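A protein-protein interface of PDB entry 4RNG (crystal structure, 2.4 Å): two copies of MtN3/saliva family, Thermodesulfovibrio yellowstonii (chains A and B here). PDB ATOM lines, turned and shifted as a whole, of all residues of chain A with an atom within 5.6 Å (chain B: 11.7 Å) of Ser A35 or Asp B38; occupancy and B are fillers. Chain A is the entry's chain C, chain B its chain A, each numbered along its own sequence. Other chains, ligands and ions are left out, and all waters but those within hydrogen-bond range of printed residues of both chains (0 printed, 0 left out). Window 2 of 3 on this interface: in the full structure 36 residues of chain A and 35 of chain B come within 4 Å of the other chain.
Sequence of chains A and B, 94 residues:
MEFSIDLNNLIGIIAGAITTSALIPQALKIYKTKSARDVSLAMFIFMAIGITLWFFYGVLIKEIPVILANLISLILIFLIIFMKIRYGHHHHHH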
ATOM      1  N   GLN A  26       5.710   6.318 -24.207  1.00  0.00           N
ATOM      2  CA  GLN A  26       4.359   6.446 -23.675  1.00  0.00           C
ATOM      3  C   GLN A  26       3.919   7.896 -23.828  1.00  0.00           C
ATOM      4  O   GLN A  26       2.787   8.181 -24.214  1.00  0.00           O
ATOM      5  CB  GLN A  26       4.274   6.000 -22.209  1.00  0.00           C
ATOM      6  CG  GLN A  26       2.864   5.992 -21.659  1.00  0.00           C
ATOM      7  CD  GLN A  26       1.950   4.987 -22.352  1.00  0.00           C
ATOM      8  OE1 GLN A  26       1.986   3.797 -22.040  1.00  0.00           O
ATOM      9  NE2 GLN A  26       1.119   5.461 -23.287  1.00  0.00           N
ATOM     10  N   LYS A  29       3.177   8.673 -27.583  1.00  0.00           N
ATOM     11  CA  LYS A  29       1.968   8.013 -28.046  1.00  0.00           C
ATOM     12  C   LYS A  29       0.726   8.797 -27.642  1.00  0.00           C
ATOM     13  O   LYS A  29      -0.186   9.003 -28.450  1.00  0.00           O
ATOM     14  CB  LYS A  29       1.909   6.588 -27.502  1.00  0.00           C
ATOM     15  CG  LYS A  29       0.780   5.752 -28.026  1.00  0.00           C
ATOM     16  CD  LYS A  29       0.863   4.375 -27.415  1.00  0.00           C
ATOM     17  CE  LYS A  29      -0.302   3.514 -27.845  1.00  0.00           C
ATOM     18  NZ  LYS A  29       0.126   2.148 -28.246  1.00  0.00           N
ATOM     19  N   ILE A  30       0.698   9.236 -26.390  1.00  0.00           N
ATOM     20  CA  ILE A  30      -0.410  10.039 -25.908  1.00  0.00           C
ATOM     21  C   ILE A  30      -0.495  11.328 -26.713  1.00  0.00           C
ATOM     22  O   ILE A  30      -1.572  11.730 -27.138  1.00  0.00           O
ATOM     23  CB  ILE A  30      -0.260  10.348 -24.408  1.00  0.00           C
ATOM     24  CG1 ILE A  30      -0.401   9.054 -23.604  1.00  0.00           C
ATOM     25  CG2 ILE A  30      -1.307  11.347 -23.965  1.00  0.00           C
ATOM     26  CD1 ILE A  30      -0.112   9.214 -22.131  1.00  0.00           C
ATOM     27  N   THR A  33      -1.606  10.708 -30.493  1.00  0.00           N
ATOM     28  CA  THR A  33      -3.012  10.323 -30.630  1.00  0.00           C
ATOM     29  C   THR A  33      -3.959  11.206 -29.824  1.00  0.00           C
ATOM     30  O   THR A  33      -5.172  11.127 -29.998  1.00  0.00           O
ATOM     31  CB  THR A  33      -3.251   8.877 -30.197  1.00  0.00           C
ATOM     32  OG1 THR A  33      -3.051   8.759 -28.780  1.00  0.00           O
ATOM     33  CG2 THR A  33      -2.308   7.941 -30.939  1.00  0.00           C
ATOM     34  N   LYS A  34      -3.410  12.036 -28.940  1.00  0.00           N
ATOM     35  CA  LYS A  34      -4.229  12.935 -28.124  1.00  0.00           C
ATOM     36  C   LYS A  34      -5.264  12.180 -27.272  1.00  0.00           C
ATOM     37  O   LYS A  34      -6.342  12.695 -26.979  1.00  0.00           O
ATOM     38  CB  LYS A  34      -4.949  13.955 -29.031  1.00  0.00           C
ATOM     39  CG  LYS A  34      -4.041  14.668 -30.039  1.00  0.00           C
ATOM     40  CD  LYS A  34      -3.247  15.753 -29.338  1.00  0.00           C
ATOM     41  CE  LYS A  34      -2.250  16.425 -30.264  1.00  0.00           C
ATOM     42  NZ  LYS A  34      -1.324  17.276 -29.464  1.00  0.00           N
ATOM     43  N   SER A  35      -4.946  10.951 -26.889  1.00  0.00           N
ATOM     44  CA  SER A  35      -5.855  10.166 -26.066  1.00  0.00           C
ATOM     45  C   SER A  35      -5.077   9.323 -25.063  1.00  0.00           C
ATOM     46  O   SER A  35      -4.014   8.806 -25.381  1.00  0.00           O
ATOM     47  CB  SER A  35      -6.740   9.270 -26.931  1.00  0.00           C
ATOM     48  OG  SER A  35      -5.996   8.184 -27.434  1.00  0.00           O
ATOM     49  N   ALA A  36      -5.590   9.203 -23.846  1.00  0.00           N
ATOM     50  CA  ALA A  36      -4.903   8.412 -22.836  1.00  0.00           C
ATOM     51  C   ALA A  36      -5.924   7.697 -21.957  1.00  0.00           C
ATOM     52  O   ALA A  36      -5.661   7.379 -20.803  1.00  0.00           O
ATOM     53  CB  ALA A  36      -3.956   9.294 -21.991  1.00  0.00           C
ATOM     54  N   ARG A  37      -7.083   7.418 -22.528  1.00  0.00           N
ATOM     55  CA  ARG A  37      -8.162   6.804 -21.773  1.00  0.00           C
ATOM     56  C   ARG A  37      -7.697   5.545 -21.069  1.00  0.00           C
ATOM     57  O   ARG A  37      -7.983   5.367 -19.893  1.00  0.00           O
ATOM     58  CB  ARG A  37      -9.351   6.493 -22.699  1.00  0.00           C
ATOM     59  CG  ARG A  37     -10.259   5.356 -22.213  1.00  0.00           C
ATOM     60  CD  ARG A  37     -11.774   5.561 -22.410  1.00  0.00           C
ATOM     61  NE  ARG A  37     -12.368   6.588 -21.546  1.00  0.00           N
ATOM     62  CZ  ARG A  37     -13.635   6.998 -21.630  1.00  0.00           C
ATOM     63  NH1 ARG A  37     -14.450   6.487 -22.549  1.00  0.00           N
ATOM     64  NH2 ARG A  37     -14.091   7.921 -20.791  1.00  0.00           N
ATOM     65  N   ASP A  38      -6.958   4.696 -21.781  1.00  0.00           N
ATOM     66  CA  ASP A  38      -6.568   3.383 -21.266  1.00  0.00           C
ATOM     67  C   ASP A  38      -5.360   3.432 -20.328  1.00  0.00           C
ATOM     68  O   ASP A  38      -5.097   2.478 -19.608  1.00  0.00           O
ATOM     69  CB  ASP A  38      -6.276   2.422 -22.419  1.00  0.00           C
ATOM     70  CG  ASP A  38      -7.451   2.279 -23.366  1.00  0.00           C
ATOM     71  OD1 ASP A  38      -8.589   2.136 -22.874  1.00  0.00           O
ATOM     72  OD2 ASP A  38      -7.242   2.321 -24.600  1.00  0.00           O
ATOM     73  N   VAL A  39      -4.638   4.543 -20.340  1.00  0.00           N
ATOM     74  CA  VAL A  39      -3.460   4.725 -19.495  1.00  0.00           C
ATOM     75  C   VAL A  39      -3.867   4.924 -18.036  1.00  0.00           C
ATOM     76  O   VAL A  39      -4.832   5.635 -17.761  1.00  0.00           O
ATOM     77  CB  VAL A  39      -2.643   5.938 -19.952  1.00  0.00           C
ATOM     78  CG1 VAL A  39      -1.420   6.074 -19.103  1.00  0.00           C
ATOM     79  CG2 VAL A  39      -2.245   5.793 -21.412  1.00  0.00           C
ATOM     80  N   TYR A  87      -5.931  15.585 -22.083  1.00  0.00           N
ATOM     81  CA  TYR A  87      -6.708  14.893 -23.107  1.00  0.00           C
ATOM     82  C   TYR A  87      -7.888  14.140 -22.545  1.00  0.00           C
ATOM     83  O   TYR A  87      -8.690  13.587 -23.291  1.00  0.00           O
ATOM     84  CB  TYR A  87      -5.806  13.949 -23.905  1.00  0.00           C
ATOM     85  CG  TYR A  87      -4.704  14.680 -24.641  1.00  0.00           C
ATOM     86  CD1 TYR A  87      -4.982  15.843 -25.353  1.00  0.00           C
ATOM     87  CD2 TYR A  87      -3.386  14.245 -24.584  1.00  0.00           C
ATOM     88  CE1 TYR A  87      -3.986  16.531 -26.023  1.00  0.00           C
ATOM     89  CE2 TYR A  87      -2.370  14.939 -25.243  1.00  0.00           C
ATOM     90  CZ  TYR A  87      -2.682  16.078 -25.962  1.00  0.00           C
ATOM     91  OH  TYR A  87      -1.691  16.763 -26.627  1.00  0.00           O
ATOM     92  N   GLN B  26      -2.189  -0.367 -13.327  1.00  0.00           N
ATOM     93  CA  GLN B  26      -2.225  -0.418 -14.785  1.00  0.00           C
ATOM     94  C   GLN B  26      -2.681  -1.786 -15.281  1.00  0.00           C
ATOM     95  O   GLN B  26      -3.440  -1.873 -16.246  1.00  0.00           O
ATOM     96  CB  GLN B  26      -0.863  -0.070 -15.388  1.00  0.00           C
ATOM     97  CG  GLN B  26      -0.883  -0.031 -16.920  1.00  0.00           C
ATOM     98  CD  GLN B  26      -1.801   1.037 -17.453  1.00  0.00           C
ATOM     99  OE1 GLN B  26      -1.429   2.212 -17.527  1.00  0.00           O
ATOM    100  NE2 GLN B  26      -3.026   0.653 -17.774  1.00  0.00           N
ATOM    101  N   LYS B  29      -6.471  -2.064 -14.521  1.00  0.00           N
ATOM    102  CA  LYS B  29      -7.254  -1.193 -15.408  1.00  0.00           C
ATOM    103  C   LYS B  29      -7.469  -1.872 -16.764  1.00  0.00           C
ATOM    104  O   LYS B  29      -8.573  -1.868 -17.302  1.00  0.00           O
ATOM    105  CB  LYS B  29      -6.573   0.188 -15.590  1.00  0.00           C
ATOM    106  CG  LYS B  29      -7.405   1.240 -16.363  1.00  0.00           C
ATOM    107  CD  LYS B  29      -6.651   2.547 -16.515  1.00  0.00           C
ATOM    108  CE  LYS B  29      -7.397   3.556 -17.363  1.00  0.00           C
ATOM    109  NZ  LYS B  29      -8.348   4.387 -16.594  1.00  0.00           N
ATOM    110  N   ILE B  30      -6.414  -2.456 -17.314  1.00  0.00           N
ATOM    111  CA  ILE B  30      -6.556  -3.171 -18.575  1.00  0.00           C
ATOM    112  C   ILE B  30      -7.528  -4.333 -18.396  1.00  0.00           C
ATOM    113  O   ILE B  30      -8.394  -4.557 -19.228  1.00  0.00           O
ATOM    114  CB  ILE B  30      -5.203  -3.730 -19.112  1.00  0.00           C
ATOM    115  CG1 ILE B  30      -4.195  -2.619 -19.408  1.00  0.00           C
ATOM    116  CG2 ILE B  30      -5.430  -4.563 -20.338  1.00  0.00           C
ATOM    117  CD1 ILE B  30      -2.821  -3.135 -19.807  1.00  0.00           C
ATOM    118  N   THR B  33     -11.298  -2.900 -17.872  1.00  0.00           N
ATOM    119  CA  THR B  33     -11.916  -2.216 -18.996  1.00  0.00           C
ATOM    120  C   THR B  33     -11.737  -3.040 -20.249  1.00  0.00           C
ATOM    121  O   THR B  33     -12.342  -2.757 -21.268  1.00  0.00           O
ATOM    122  CB  THR B  33     -11.315  -0.845 -19.230  1.00  0.00           C
ATOM    123  OG1 THR B  33      -9.965  -1.003 -19.653  1.00  0.00           O
ATOM    124  CG2 THR B  33     -11.355  -0.021 -17.958  1.00  0.00           C
ATOM    125  N   LYS B  34     -10.898  -4.065 -20.153  1.00  0.00           N
ATOM    126  CA  LYS B  34     -10.586  -4.961 -21.264  1.00  0.00           C
ATOM    127  C   LYS B  34      -9.995  -4.202 -22.460  1.00  0.00           C
ATOM    128  O   LYS B  34     -10.174  -4.590 -23.617  1.00  0.00           O
ATOM    129  CB  LYS B  34     -11.848  -5.712 -21.686  1.00  0.00           C
ATOM    130  CG  LYS B  34     -12.516  -6.504 -20.555  1.00  0.00           C
ATOM    131  CD  LYS B  34     -11.838  -7.827 -20.230  1.00  0.00           C
ATOM    132  CE  LYS B  34     -12.530  -8.495 -19.021  1.00  0.00           C
ATOM    133  NZ  LYS B  34     -11.784  -9.665 -18.454  1.00  0.00           N
ATOM    134  N   SER B  35      -9.298  -3.109 -22.183  1.00  0.00           N
ATOM    135  CA  SER B  35      -8.716  -2.333 -23.258  1.00  0.00           C
ATOM    136  C   SER B  35      -7.377  -1.745 -22.856  1.00  0.00           C
ATOM    137  O   SER B  35      -7.201  -1.266 -21.740  1.00  0.00           O
ATOM    138  CB  SER B  35      -9.676  -1.239 -23.712  1.00  0.00           C
ATOM    139  OG  SER B  35      -9.717  -0.226 -22.753  1.00  0.00           O
ATOM    140  N   ALA B  36      -6.451  -1.748 -23.805  1.00  0.00           N
ATOM    141  CA  ALA B  36      -5.102  -1.299 -23.565  1.00  0.00           C
ATOM    142  C   ALA B  36      -4.551  -0.541 -24.758  1.00  0.00           C
ATOM    143  O   ALA B  36      -3.337  -0.473 -24.933  1.00  0.00           O
ATOM    144  CB  ALA B  36      -4.214  -2.505 -23.254  1.00  0.00           C
ATOM    145  N   ARG B  37      -5.442   0.051 -25.551  1.00  0.00           N
ATOM    146  CA  ARG B  37      -5.047   0.746 -26.779  1.00  0.00           C
ATOM    147  C   ARG B  37      -4.003   1.844 -26.517  1.00  0.00           C
ATOM    148  O   ARG B  37      -2.950   1.857 -27.144  1.00  0.00           O
ATOM    149  CB  ARG B  37      -6.272   1.381 -27.451  1.00  0.00           C
ATOM    150  CG  ARG B  37      -5.921   2.343 -28.569  1.00  0.00           C
ATOM    151  CD  ARG B  37      -7.132   3.002 -29.236  1.00  0.00           C
ATOM    152  NE  ARG B  37      -8.019   2.093 -29.952  1.00  0.00           N
ATOM    153  CZ  ARG B  37      -9.174   2.464 -30.504  1.00  0.00           C
ATOM    154  NH1 ARG B  37      -9.578   3.730 -30.439  1.00  0.00           N
ATOM    155  NH2 ARG B  37      -9.922   1.572 -31.138  1.00  0.00           N
ATOM    156  N   ASP B  38      -4.248   2.706 -25.534  1.00  0.00           N
ATOM    157  CA  ASP B  38      -3.404   3.882 -25.353  1.00  0.00           C
ATOM    158  C   ASP B  38      -2.105   3.546 -24.638  1.00  0.00           C
ATOM    159  O   ASP B  38      -1.162   4.326 -24.655  1.00  0.00           O
ATOM    160  CB  ASP B  38      -4.143   4.963 -24.558  1.00  0.00           C
ATOM    161  CG  ASP B  38      -5.468   5.329 -25.163  1.00  0.00           C
ATOM    162  OD1 ASP B  38      -5.529   5.496 -26.402  1.00  0.00           O
ATOM    163  OD2 ASP B  38      -6.448   5.441 -24.393  1.00  0.00           O
ATOM    164  N   VAL B  39      -2.067   2.379 -24.011  1.00  0.00           N
ATOM    165  CA  VAL B  39      -0.900   1.946 -23.260  1.00  0.00           C
ATOM    166  C   VAL B  39       0.194   1.610 -24.253  1.00  0.00           C
ATOM    167  O   VAL B  39      -0.072   0.983 -25.282  1.00  0.00           O
ATOM    168  CB  VAL B  39      -1.234   0.721 -22.354  1.00  0.00           C
ATOM    169  CG1 VAL B  39      -0.021   0.215 -21.635  1.00  0.00           C
ATOM    170  CG2 VAL B  39      -2.317   1.069 -21.362  1.00  0.00           C
ATOM    171  N   SER B  40       1.415   2.048 -23.970  1.00  0.00           N
ATOM    172  CA  SER B  40       2.516   1.822 -24.888  1.00  0.00           C
ATOM    173  C   SER B  40       3.237   0.499 -24.620  1.00  0.00           C
ATOM    174  O   SER B  40       3.752   0.296 -23.524  1.00  0.00           O
ATOM    175  CB  SER B  40       3.508   2.966 -24.797  1.00  0.00           C
ATOM    176  OG  SER B  40       4.703   2.636 -25.485  1.00  0.00           O
ATOM    177  N   LEU B  41       3.280  -0.403 -25.598  1.00  0.00           N
ATOM    178  CA  LEU B  41       3.959  -1.678 -25.374  1.00  0.00           C
ATOM    179  C   LEU B  41       5.459  -1.440 -25.306  1.00  0.00           C
ATOM    180  O   LEU B  41       6.159  -2.033 -24.477  1.00  0.00           O
ATOM    181  CB  LEU B  41       3.625  -2.705 -26.459  1.00  0.00           C
ATOM    182  CG  LEU B  41       4.190  -4.129 -26.291  1.00  0.00           C
ATOM    183  CD1 LEU B  41       3.683  -4.835 -25.033  1.00  0.00           C
ATOM    184  CD2 LEU B  41       3.906  -4.982 -27.503  1.00  0.00           C
ATOM    185  N   ALA B  42       5.944  -0.532 -26.143  1.00  0.00           N
ATOM    186  CA  ALA B  42       7.363  -0.204 -26.147  1.00  0.00           C
ATOM    187  C   ALA B  42       7.841   0.216 -24.774  1.00  0.00           C
ATOM    188  O   ALA B  42       8.866  -0.272 -24.332  1.00  0.00           O
ATOM    189  CB  ALA B  42       7.664   0.893 -27.161  1.00  0.00           C
ATOM    190  N   MET B  43       7.103   1.103 -24.101  1.00  0.00           N
ATOM    191  CA  MET B  43       7.492   1.566 -22.759  1.00  0.00           C
ATOM    192  C   MET B  43       7.758   0.403 -21.805  1.00  0.00           C
ATOM    193  O   MET B  43       8.753   0.415 -21.082  1.00  0.00           O
ATOM    194  CB  MET B  43       6.446   2.499 -22.130  1.00  0.00           C
ATOM    195  CG  MET B  43       6.707   2.755 -20.626  1.00  0.00           C
ATOM    196  SD  MET B  43       5.457   3.727 -19.730  1.00  0.00           S
ATOM    197  CE  MET B  43       5.843   3.354 -18.023  1.00  0.00           C
ATOM    198  N   PHE B  44       6.882  -0.599 -21.798  1.00  0.00           N
ATOM    199  CA  PHE B  44       7.026  -1.687 -20.827  1.00  0.00           C
ATOM    200  C   PHE B  44       8.098  -2.696 -21.214  1.00  0.00           C
ATOM    201  O   PHE B  44       8.796  -3.234 -20.351  1.00  0.00           O
ATOM    202  CB  PHE B  44       5.687  -2.371 -20.619  1.00  0.00           C
ATOM    203  CG  PHE B  44       4.778  -1.558 -19.791  1.00  0.00           C
ATOM    204  CD1 PHE B  44       4.991  -1.452 -18.436  1.00  0.00           C
ATOM    205  CD2 PHE B  44       3.761  -0.829 -20.376  1.00  0.00           C
ATOM    206  CE1 PHE B  44       4.190  -0.678 -17.673  1.00  0.00           C
ATOM    207  CE2 PHE B  44       2.945  -0.041 -19.619  1.00  0.00           C
ATOM    208  CZ  PHE B  44       3.158   0.037 -18.258  1.00  0.00           C
ATOM    209  N   ILE B  80       1.707  -7.040 -16.930  1.00  0.00           N
ATOM    210  CA  ILE B  80       1.126  -5.947 -17.707  1.00  0.00           C
ATOM    211  C   ILE B  80       1.289  -6.222 -19.203  1.00  0.00           C
ATOM    212  O   ILE B  80       0.329  -6.086 -19.975  1.00  0.00           O
ATOM    213  CB  ILE B  80       1.773  -4.572 -17.370  1.00  0.00           C
ATOM    214  CG1 ILE B  80       1.370  -4.113 -15.970  1.00  0.00           C
ATOM    215  CG2 ILE B  80       1.357  -3.514 -18.371  1.00  0.00           C
ATOM    216  CD1 ILE B  80       2.222  -2.997 -15.421  1.00  0.00           C
ATOM    217  N   MET B  83      -1.313  -8.633 -20.453  1.00  0.00           N
ATOM    218  CA  MET B  83      -2.655  -8.113 -20.671  1.00  0.00           C
ATOM    219  C   MET B  83      -2.731  -7.049 -21.757  1.00  0.00           C
ATOM    220  O   MET B  83      -3.774  -6.881 -22.386  1.00  0.00           O
ATOM    221  CB  MET B  83      -3.233  -7.653 -19.356  1.00  0.00           C
ATOM    222  CG  MET B  83      -3.703  -8.888 -18.657  1.00  0.00           C
ATOM    223  SD  MET B  83      -4.447  -8.513 -17.129  1.00  0.00           S
ATOM    224  CE  MET B  83      -3.032  -7.755 -16.352  1.00  0.00           C
ATOM    225  N   LYS B  84      -1.643  -6.331 -21.979  1.00  0.00           N
ATOM    226  CA  LYS B  84      -1.603  -5.446 -23.127  1.00  0.00           C
ATOM    227  C   LYS B  84      -1.879  -6.221 -24.426  1.00  0.00           C
ATOM    228  O   LYS B  84      -2.660  -5.798 -25.284  1.00  0.00           O
ATOM    229  CB  LYS B  84      -0.251  -4.743 -23.190  1.00  0.00           C
ATOM    230  CG  LYS B  84       0.010  -4.024 -24.497  1.00  0.00           C
ATOM    231  CD  LYS B  84      -0.797  -2.778 -24.687  1.00  0.00           C
ATOM    232  CE  LYS B  84      -0.314  -2.091 -25.947  1.00  0.00           C
ATOM    233  NZ  LYS B  84      -1.360  -1.241 -26.577  1.00  0.00           N
ATOM    234  N   ILE B  85      -1.250  -7.374 -24.546  1.00  0.00           N
ATOM    235  CA  ILE B  85      -1.398  -8.202 -25.717  1.00  0.00           C
ATOM    236  C   ILE B  85      -2.734  -8.912 -25.810  1.00  0.00           C
ATOM    237  O   ILE B  85      -3.280  -9.070 -26.891  1.00  0.00           O
ATOM    238  CB  ILE B  85      -0.286  -9.238 -25.758  1.00  0.00           C
ATOM    239  CG1 ILE B  85       1.064  -8.538 -25.602  1.00  0.00           C
ATOM    240  CG2 ILE B  85      -0.368 -10.060 -27.048  1.00  0.00           C
ATOM    241  CD1 ILE B  85       2.191  -9.491 -25.372  1.00  0.00           C
ATOM    242  N   TYR B  87      -5.558  -7.835 -24.756  1.00  0.00           N
ATOM    243  CA  TYR B  87      -6.528  -6.811 -25.130  1.00  0.00           C
ATOM    244  C   TYR B  87      -5.942  -5.843 -26.168  1.00  0.00           C
ATOM    245  O   TYR B  87      -6.111  -4.625 -26.097  1.00  0.00           O
ATOM    246  CB  TYR B  87      -6.988  -6.082 -23.881  1.00  0.00           C
ATOM    247  CG  TYR B  87      -7.541  -7.047 -22.855  1.00  0.00           C
ATOM    248  CD1 TYR B  87      -8.686  -7.778 -23.111  1.00  0.00           C
ATOM    249  CD2 TYR B  87      -6.881  -7.265 -21.656  1.00  0.00           C
ATOM    250  CE1 TYR B  87      -9.179  -8.666 -22.183  1.00  0.00           C
ATOM    251  CE2 TYR B  87      -7.362  -8.147 -20.724  1.00  0.00           C
ATOM    252  CZ  TYR B  87      -8.510  -8.847 -20.983  1.00  0.00           C
ATOM    253  OH  TYR B  87      -8.978  -9.727 -20.026  1.00  0.00           O
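The backbone carbonyl oxygen (O) of Asp A38 lies within hydrogen-bond range of the side-chain amide nitrogen (NE2) of Gln B26 (3.3 Å).
The side-chain amino group (NZ) of Lys B29 lies close to the backbone carbonyl oxygen (O) of Arg A37, at 3.5 Å.
The side-chain carboxylate of Asp A38 sits at hydrogen-bond distance from the side-chain hydroxyl of Ser B35 (2.6 Å).
NZ of Lys A29 sits close to O of Arg B37 (3.3 Å).
The backbone NH (N) of Arg B37 sits at hydrogen-bond distance from the side-chain carboxylate (OD2) of Asp A38, 3.0 Å away.
The side-chain amide nitrogen (NE2) of Gln A26 lies within hydrogen-bond range of the backbone carbonyl oxygen (O) of Asp B38, at 2.9 Å.
The side-chain hydroxyl (OG) of Ser A35 is in hydrogen-bond range of the side-chain carboxylate (OD1) of Asp B38 (2.9 Å).
OD2 of Asp B38 lies within hydrogen-bond range of N of Arg A37, 2.8 Å away.
The side-chain carboxylate (OD2) of Asp B38 sits at hydrogen-bond distance from the backbone NH (N) of Asp A38 (2.8 Å).
The side-chain amino group of Lys A29 sits at hydrogen-bond distance from the backbone carbonyl oxygen of Val B39.
N of Ser B40 is in hydrogen-bond range of OE1 of Gln A26.
O of Lys B29 sits at hydrogen-bond distance from OG1 of Thr B33, 2.9 Å away.
The backbone NH (N) of Ser B35 sits at hydrogen-bond distance from the backbone carbonyl oxygen (O) of Ile B30 (3.4 Å).
The side-chain amino group (NZ) of Lys B84 lies within hydrogen-bond range of the backbone carbonyl oxygen (O) of Val B39, at 2.9 Å.
The backbone NH (N) of Ala B42 lies close to the side-chain hydroxyl (OG) of Ser B40.
N of Met B43 sits at hydrogen-bond distance from OG of Ser B40 (3.2 Å).
The side-chain hydroxyl (OG) of Ser A35 lies within hydrogen-bond range of the side-chain hydroxyl (OG1) of Thr A33 (3.3 Å).
Gln A26 touches Val B39.
O of Asp B38 touches CE of Lys A29, 3.4 Å away.
CD of Lys A29 touches CA of Ser B40 (3.95 Å).
Asp B38 touches Ala A36.
Lys B29 touches Asp A38.
C of Ala B36 touches OD2 of Asp A38, at 3.9 Å.
O of Asp A38 touches CG2 of Val B39 (3.6 Å).
C of Val A39 touches OE1 of Gln B26, 3.7 Å away.
Lys B29 touches Val A39 (CE to O, 3.3 Å).
Val A39 touches Asp B38.
Lys A29 touches just these residues of chain B: Arg B37 (3.2 Å), Asp B38 (3.4 Å), Val B39 (3.2 Å) and Ser B40 (3.95 Å).
No residue of chain B comes within 4 Å of Thr A33.
Ser A35 touches one residue of chain B.
Printed residues of chain B within 4 Å of Arg A37: Lys B29 (3.2 Å) and Asp B38 (2.8 Å).
Of chain B, only Gln B26 (3.3 Å), Lys B29 (3.4 Å), Ser B35 (2.6 Å), Ala B36 (3.9 Å), Arg B37 (3.0 Å), Asp B38 (2.8 Å) and Val B39 (3.6 Å) come within 4 Å of Asp A38.
Val A39 touches three residues of chain B.
Tyr A87 touches none of the printed residues of chain B.
Of the printed residues of chain A, Lys B29 touches Arg A37, Asp A38 and Val A39.
Printed residues of chain A within 4 Å of Ala B36: Asp A38 (3.9 Å).
Asp B38 touches just these residues of chain A: Gln A26 (2.9 Å), Lys A29 (3.4 Å), Ser A35 (2.9 Å), Ala A36 (3.4 Å), Arg A37 (2.8 Å), Asp A38 (2.8 Å) and Val A39 (3.7 Å).
Of the printed residues of chain A, Val B39 touches Gln A26, Lys A29 and Asp A38.
Ala B42 touches none of the printed residues of chain A.
Of the printed residues of chain A, Met B43 touches Gln A26 (3.6 Å).
Ile B85 touches none of the printed residues of chain A.
Along chain A the printed residues that touch a printed residue of chain B span positions 26 to 39.
Of the 20 printed residues of chain B, 9 touch a printed residue of chain A.
Gln A26 touches Asp B38, and with the chains exchanged Asp A38 touches Gln B26.
Gln A26 touches Val B39, and with the chains exchanged Val A39 touches Gln B26.
Lys A29 touches Asp B38, and with the chains exchanged Asp A38 touches Lys B29.
Asp A38 touches Val B39, and with the chains exchanged Val A39 touches Asp B38.
11 positions are printed for both chains.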
